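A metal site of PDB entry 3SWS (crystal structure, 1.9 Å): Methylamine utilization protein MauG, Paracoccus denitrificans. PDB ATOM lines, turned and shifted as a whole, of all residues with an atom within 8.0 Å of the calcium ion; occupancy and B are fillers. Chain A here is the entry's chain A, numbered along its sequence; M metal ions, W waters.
O of Asn 66 is in hydrogen-bond range of NE1 of Trp 93, at 2.9 Å. N of Asn 66 is in hydrogen-bond range of O of His 280, 2.8 Å away. The side-chain amide nitrogen of Asn 66 is in hydrogen-bond range of the backbone carbonyl oxygen of Leu 51, 3.3 Å away. The backbone carbonyl oxygen of Ala 52 sits at hydrogen-bond distance from the side-chain amide nitrogen of Asn 66 (2.9 Å). OG1 of Thr 275 sits at hydrogen-bond distance from O of Val 272 (3.5 Å). The side-chain hydroxyl (OG1) of Thr 275 lies close to the backbone carbonyl oxygen (O) of Asn 271, at 3.4 Å.
Of the 23 residues printed, 3 come within 4 Å of the calcium ion. The nearest printed residue that does not touch the calcium ion is Gly 276 (4.1 Å).
The calcium ion is bound by water W1 (2.3 Å), the backbone carbonyl oxygen (O) of Thr 275 (2.3 Å), the backbone carbonyl oxygen (O) of Pro 277 (2.4 Å), water W3 (2.4 Å), the side-chain amide oxygen (OD1) of Asn 66 (2.4 Å), water W4 (2.4 Å) and water W2 (2.6 Å).
Water W2 lies within hydrogen-bond range of O of Gly 276 (2.9 Å) and ND2 of Asn 66 (3.1 Å).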
ATOM      1  N   ARG A  39      -5.355 -10.550  19.323  1.00  0.00           N
ATOM      2  CA  ARG A  39      -5.061  -9.930  20.656  1.00  0.00           C
ATOM      3  C   ARG A  39      -3.661  -9.305  20.641  1.00  0.00           C
ATOM      4  O   ARG A  39      -2.847  -9.489  21.566  1.00  0.00           O
ATOM      5  CB  ARG A  39      -5.252 -10.975  21.773  1.00  0.00           C
ATOM      6  CG  ARG A  39      -5.604 -10.314  23.146  1.00  0.00           C
ATOM      7  CD  ARG A  39      -5.411 -11.347  24.282  1.00  0.00           C
ATOM      8  NE  ARG A  39      -5.924 -10.844  25.550  1.00  0.00           N
ATOM      9  CZ  ARG A  39      -5.146 -10.341  26.499  1.00  0.00           C
ATOM     10  NH1 ARG A  39      -5.704  -9.903  27.627  1.00  0.00           N
ATOM     11  NH2 ARG A  39      -3.788 -10.264  26.294  1.00  0.00           N
ATOM     12  N   THR A  42      -0.832 -12.023  21.543  1.00  0.00           N
ATOM     13  CA  THR A  42      -0.649 -12.409  22.936  1.00  0.00           C
ATOM     14  C   THR A  42      -1.706 -13.447  23.214  1.00  0.00           C
ATOM     15  O   THR A  42      -2.492 -13.741  22.308  1.00  0.00           O
ATOM     16  CB  THR A  42      -0.766 -11.209  23.979  1.00  0.00           C
ATOM     17  OG1 THR A  42      -2.091 -10.675  23.957  1.00  0.00           O
ATOM     18  CG2 THR A  42       0.250 -10.077  23.667  1.00  0.00           C
ATOM     19  N   ASP A  43      -1.691 -14.035  24.406  1.00  0.00           N
ATOM     20  CA  ASP A  43      -2.478 -15.266  24.679  1.00  0.00           C
ATOM     21  C   ASP A  43      -3.769 -14.941  25.430  1.00  0.00           C
ATOM     22  O   ASP A  43      -3.714 -14.507  26.574  1.00  0.00           O
ATOM     23  CB  ASP A  43      -1.601 -16.315  25.460  1.00  0.00           C
ATOM     24  CG  ASP A  43      -2.290 -17.689  25.622  1.00  0.00           C
ATOM     25  OD1 ASP A  43      -1.641 -18.648  26.156  1.00  0.00           O
ATOM     26  OD2 ASP A  43      -3.449 -17.811  25.164  1.00  0.00           O
ATOM     27  N   LEU A  51      -4.358 -15.190  33.058  1.00  0.00           N
ATOM     28  CA  LEU A  51      -3.739 -14.948  31.776  1.00  0.00           C
ATOM     29  C   LEU A  51      -2.292 -14.630  31.986  1.00  0.00           C
ATOM     30  O   LEU A  51      -1.629 -14.189  31.054  1.00  0.00           O
ATOM     31  CB  LEU A  51      -4.387 -13.772  31.071  1.00  0.00           C
ATOM     32  CG  LEU A  51      -5.533 -14.126  30.120  1.00  0.00           C
ATOM     33  CD1 LEU A  51      -6.713 -14.767  30.839  1.00  0.00           C
ATOM     34  CD2 LEU A  51      -5.965 -12.862  29.366  1.00  0.00           C
ATOM     35  N   ALA A  52      -1.806 -14.815  33.208  1.00  0.00           N
ATOM     36  CA  ALA A  52      -0.414 -14.413  33.468  1.00  0.00           C
ATOM     37  C   ALA A  52       0.624 -15.239  32.688  1.00  0.00           C
ATOM     38  O   ALA A  52       1.649 -14.693  32.302  1.00  0.00           O
ATOM     39  CB  ALA A  52      -0.120 -14.467  34.949  1.00  0.00           C
ATOM     40  N   ASN A  66       5.101 -14.377  31.216  1.00  0.00           N
ATOM     41  CA  ASN A  66       3.924 -13.962  30.464  1.00  0.00           C
ATOM     42  C   ASN A  66       4.251 -13.911  28.947  1.00  0.00           C
ATOM     43  O   ASN A  66       5.320 -13.438  28.572  1.00  0.00           O
ATOM     44  CB  ASN A  66       3.548 -12.543  30.956  1.00  0.00           C
ATOM     45  CG  ASN A  66       2.356 -11.939  30.224  1.00  0.00           C
ATOM     46  OD1 ASN A  66       2.485 -10.889  29.556  1.00  0.00           O
ATOM     47  ND2 ASN A  66       1.196 -12.562  30.353  1.00  0.00           N
ATOM     48  N   THR A  67       3.361 -14.380  28.074  1.00  0.00           N
ATOM     49  CA  THR A  67       3.596 -14.338  26.625  1.00  0.00           C
ATOM     50  C   THR A  67       3.565 -12.880  26.106  1.00  0.00           C
ATOM     51  O   THR A  67       2.524 -12.231  26.205  1.00  0.00           O
ATOM     52  CB  THR A  67       2.562 -15.237  25.898  1.00  0.00           C
ATOM     53  OG1 THR A  67       2.705 -16.598  26.366  1.00  0.00           O
ATOM     54  CG2 THR A  67       2.760 -15.204  24.347  1.00  0.00           C
ATOM     55  N   PRO A  68       4.707 -12.370  25.547  1.00  0.00           N
ATOM     56  CA  PRO A  68       4.811 -10.962  25.056  1.00  0.00           C
ATOM     57  C   PRO A  68       4.226 -10.880  23.631  1.00  0.00           C
ATOM     58  O   PRO A  68       4.151 -11.887  22.918  1.00  0.00           O
ATOM     59  CB  PRO A  68       6.339 -10.689  24.992  1.00  0.00           C
ATOM     60  CG  PRO A  68       6.872 -12.094  24.593  1.00  0.00           C
ATOM     61  CD  PRO A  68       5.983 -13.098  25.389  1.00  0.00           C
ATOM     62  N   THR A  69       3.755  -9.702  23.261  1.00  0.00           N
ATOM     63  CA  THR A  69       3.412  -9.422  21.857  1.00  0.00           C
ATOM     64  C   THR A  69       4.605  -9.668  20.948  1.00  0.00           C
ATOM     65  O   THR A  69       5.781  -9.493  21.363  1.00  0.00           O
ATOM     66  CB  THR A  69       2.981  -7.911  21.726  1.00  0.00           C
ATOM     67  OG1 THR A  69       2.538  -7.635  20.391  1.00  0.00           O
ATOM     68  CG2 THR A  69       4.154  -6.920  22.028  1.00  0.00           C
ATOM     69  N   TRP A  93      12.258 -12.276  27.449  1.00  0.00           N
ATOM     70  CA  TRP A  93      12.311 -11.246  28.470  1.00  0.00           C
ATOM     71  C   TRP A  93      13.714 -11.179  29.088  1.00  0.00           C
ATOM     72  O   TRP A  93      14.041 -10.145  29.635  1.00  0.00           O
ATOM     73  CB  TRP A  93      11.307 -11.597  29.601  1.00  0.00           C
ATOM     74  CG  TRP A  93       9.876 -11.369  29.310  1.00  0.00           C
ATOM     75  CD1 TRP A  93       8.953 -12.313  28.873  1.00  0.00           C
ATOM     76  CD2 TRP A  93       9.144 -10.126  29.482  1.00  0.00           C
ATOM     77  NE1 TRP A  93       7.679 -11.699  28.787  1.00  0.00           N
ATOM     78  CE2 TRP A  93       7.787 -10.380  29.174  1.00  0.00           C
ATOM     79  CE3 TRP A  93       9.510  -8.841  29.953  1.00  0.00           C
ATOM     80  CZ2 TRP A  93       6.807  -9.392  29.256  1.00  0.00           C
ATOM     81  CZ3 TRP A  93       8.553  -7.851  30.030  1.00  0.00           C
ATOM     82  CH2 TRP A  93       7.184  -8.132  29.693  1.00  0.00           C
ATOM     83  N   ASN A 271       0.750  -1.133  21.783  1.00  0.00           N
ATOM     84  CA  ASN A 271      -0.352  -2.101  22.131  1.00  0.00           C
ATOM     85  C   ASN A 271      -0.421  -2.496  23.581  1.00  0.00           C
ATOM     86  O   ASN A 271      -1.224  -3.372  23.947  1.00  0.00           O
ATOM     87  CB  ASN A 271      -0.322  -3.334  21.217  1.00  0.00           C
ATOM     88  CG  ASN A 271      -0.622  -2.968  19.751  1.00  0.00           C
ATOM     89  OD1 ASN A 271      -1.609  -2.235  19.440  1.00  0.00           O
ATOM     90  ND2 ASN A 271       0.232  -3.462  18.835  1.00  0.00           N
ATOM     91  N   VAL A 272       0.288  -1.756  24.443  1.00  0.00           N
ATOM     92  CA  VAL A 272       0.202  -2.127  25.870  1.00  0.00           C
ATOM     93  C   VAL A 272      -1.232  -2.155  26.437  1.00  0.00           C
ATOM     94  O   VAL A 272      -1.534  -2.964  27.331  1.00  0.00           O
ATOM     95  CB  VAL A 272       1.167  -1.228  26.761  1.00  0.00           C
ATOM     96  CG1 VAL A 272       0.685   0.301  26.857  1.00  0.00           C
ATOM     97  CG2 VAL A 272       1.328  -1.845  28.168  1.00  0.00           C
ATOM     98  N   VAL A 274      -3.801  -3.261  25.320  1.00  0.00           N
ATOM     99  CA  VAL A 274      -4.610  -4.473  25.021  1.00  0.00           C
ATOM    100  C   VAL A 274      -3.871  -5.782  25.303  1.00  0.00           C
ATOM    101  O   VAL A 274      -4.365  -6.876  24.911  1.00  0.00           O
ATOM    102  CB  VAL A 274      -5.150  -4.420  23.524  1.00  0.00           C
ATOM    103  CG1 VAL A 274      -5.915  -3.118  23.285  1.00  0.00           C
ATOM    104  CG2 VAL A 274      -3.974  -4.633  22.461  1.00  0.00           C
ATOM    105  N   THR A 275      -2.697  -5.714  25.951  1.00  0.00           N
ATOM    106  CA  THR A 275      -1.877  -6.937  26.138  1.00  0.00           C
ATOM    107  C   THR A 275      -1.648  -7.273  27.589  1.00  0.00           C
ATOM    108  O   THR A 275      -0.608  -7.911  27.932  1.00  0.00           O
ATOM    109  CB  THR A 275      -0.505  -6.841  25.440  1.00  0.00           C
ATOM    110  OG1 THR A 275       0.171  -5.678  25.981  1.00  0.00           O
ATOM    111  CG2 THR A 275      -0.716  -6.699  23.909  1.00  0.00           C
ATOM    112  N   GLY A 276      -2.585  -6.834  28.419  1.00  0.00           N
ATOM    113  CA  GLY A 276      -2.578  -7.240  29.863  1.00  0.00           C
ATOM    114  C   GLY A 276      -2.641  -8.790  29.980  1.00  0.00           C
ATOM    115  O   GLY A 276      -3.023  -9.460  29.038  1.00  0.00           O
ATOM    116  N   PRO A 277      -2.244  -9.369  31.117  1.00  0.00           N
ATOM    117  CA  PRO A 277      -1.665  -8.676  32.266  1.00  0.00           C
ATOM    118  C   PRO A 277      -0.194  -8.310  31.997  1.00  0.00           C
ATOM    119  O   PRO A 277       0.335  -8.575  30.914  1.00  0.00           O
ATOM    120  CB  PRO A 277      -1.795  -9.707  33.397  1.00  0.00           C
ATOM    121  CG  PRO A 277      -1.672 -11.081  32.624  1.00  0.00           C
ATOM    122  CD  PRO A 277      -2.498 -10.819  31.394  1.00  0.00           C
ATOM    123  N   TYR A 278       0.439  -7.665  32.989  1.00  0.00           N
ATOM    124  CA  TYR A 278       1.624  -6.862  32.715  1.00  0.00           C
ATOM    125  C   TYR A 278       2.846  -7.400  33.459  1.00  0.00           C
ATOM    126  O   TYR A 278       2.718  -8.112  34.500  1.00  0.00           O
ATOM    127  CB  TYR A 278       1.333  -5.378  33.051  1.00  0.00           C
ATOM    128  CG  TYR A 278       0.191  -4.852  32.160  1.00  0.00           C
ATOM    129  CD1 TYR A 278      -1.101  -4.671  32.679  1.00  0.00           C
ATOM    130  CD2 TYR A 278       0.392  -4.648  30.799  1.00  0.00           C
ATOM    131  CE1 TYR A 278      -2.133  -4.246  31.832  1.00  0.00           C
ATOM    132  CE2 TYR A 278      -0.629  -4.252  29.969  1.00  0.00           C
ATOM    133  CZ  TYR A 278      -1.847  -4.009  30.452  1.00  0.00           C
ATOM    134  OH  TYR A 278      -2.819  -3.587  29.574  1.00  0.00           O
ATOM    135  N   MET A 279       4.006  -6.970  32.954  1.00  0.00           N
ATOM    136  CA  MET A 279       5.363  -7.322  33.474  1.00  0.00           C
ATOM    137  C   MET A 279       5.680  -8.745  33.034  1.00  0.00           C
ATOM    138  O   MET A 279       4.825  -9.419  32.464  1.00  0.00           O
ATOM    139  CB  MET A 279       5.439  -7.203  34.967  1.00  0.00           C
ATOM    140  CG  MET A 279       5.117  -5.728  35.413  1.00  0.00           C
ATOM    141  SD  MET A 279       6.105  -4.482  34.561  1.00  0.00           S
ATOM    142  CE  MET A 279       5.264  -3.053  35.313  1.00  0.00           C
ATOM    143  N   HIS A 280       6.929  -9.172  33.304  1.00  0.00           N
ATOM    144  CA  HIS A 280       7.492 -10.431  32.771  1.00  0.00           C
ATOM    145  C   HIS A 280       6.734 -11.632  33.274  1.00  0.00           C
ATOM    146  O   HIS A 280       6.801 -12.697  32.666  1.00  0.00           O
ATOM    147  CB  HIS A 280       9.015 -10.498  33.097  1.00  0.00           C
ATOM    148  CG  HIS A 280       9.317 -10.623  34.540  1.00  0.00           C
ATOM    149  ND1 HIS A 280       9.762  -9.577  35.292  1.00  0.00           N
ATOM    150  CD2 HIS A 280       9.219 -11.681  35.360  1.00  0.00           C
ATOM    151  CE1 HIS A 280       9.880  -9.960  36.548  1.00  0.00           C
ATOM    152  NE2 HIS A 280       9.630 -11.262  36.602  1.00  0.00           N
ATOM    153  N   ASN A 281       6.040 -11.484  34.390  1.00  0.00           N
ATOM    154  CA  ASN A 281       5.343 -12.630  35.028  1.00  0.00           C
ATOM    155  C   ASN A 281       3.832 -12.351  35.113  1.00  0.00           C
ATOM    156  O   ASN A 281       3.111 -13.083  35.786  1.00  0.00           O
ATOM    157  CB  ASN A 281       5.883 -12.898  36.463  1.00  0.00           C
ATOM    158  CG  ASN A 281       5.850 -11.642  37.328  1.00  0.00           C
ATOM    159  OD1 ASN A 281       5.171 -10.637  36.997  1.00  0.00           O
ATOM    160  ND2 ASN A 281       6.567 -11.694  38.464  1.00  0.00           N
ATOM    161  N   GLY A 282       3.342 -11.329  34.398  1.00  0.00           N
ATOM    162  CA  GLY A 282       1.885 -11.141  34.285  1.00  0.00           C
ATOM    163  C   GLY A 282       1.226 -10.781  35.623  1.00  0.00           C
ATOM    164  O   GLY A 282       0.020 -11.015  35.842  1.00  0.00           O
ATOM    165  N   VAL A 283       2.043 -10.314  36.574  1.00  0.00           N
ATOM    166  CA  VAL A 283       1.544 -10.076  37.918  1.00  0.00           C
ATOM    167  C   VAL A 283       0.375  -9.004  38.049  1.00  0.00           C
ATOM    168  O   VAL A 283      -0.535  -9.165  38.894  1.00  0.00           O
ATOM    169  CB  VAL A 283       2.721  -9.787  38.899  1.00  0.00           C
ATOM    170  CG1 VAL A 283       3.445  -8.397  38.510  1.00  0.00           C
ATOM    171  CG2 VAL A 283       2.235  -9.913  40.392  1.00  0.00           C
ATOM    172  N   PHE A 284       0.364  -7.949  37.228  1.00  0.00           N
ATOM    173  CA  PHE A 284      -0.690  -6.925  37.354  1.00  0.00           C
ATOM    174  C   PHE A 284      -1.670  -7.058  36.218  1.00  0.00           C
ATOM    175  O   PHE A 284      -1.276  -7.107  35.027  1.00  0.00           O
ATOM    176  CB  PHE A 284      -0.088  -5.486  37.330  1.00  0.00           C
ATOM    177  CG  PHE A 284       1.062  -5.306  38.272  1.00  0.00           C
ATOM    178  CD1 PHE A 284       0.955  -5.768  39.609  1.00  0.00           C
ATOM    179  CD2 PHE A 284       2.233  -4.650  37.843  1.00  0.00           C
ATOM    180  CE1 PHE A 284       2.008  -5.633  40.513  1.00  0.00           C
ATOM    181  CE2 PHE A 284       3.242  -4.449  38.757  1.00  0.00           C
ATOM    182  CZ  PHE A 284       3.180  -4.970  40.077  1.00  0.00           C
HETATM  183 CA    CA M   1       1.303  -8.912  28.794  1.00  0.00          CA
HETATM  184  O   HOH W   1       1.944  -9.449  26.647  1.00  0.00           O
HETATM  185  O   HOH W   2      -0.487 -10.743  28.462  1.00  0.00           O
HETATM  186  O   HOH W   3       3.386  -8.315  29.876  1.00  0.00           O
HETATM  187  O   HOH W   4       1.844  -6.653  28.036  1.00  0.00           O
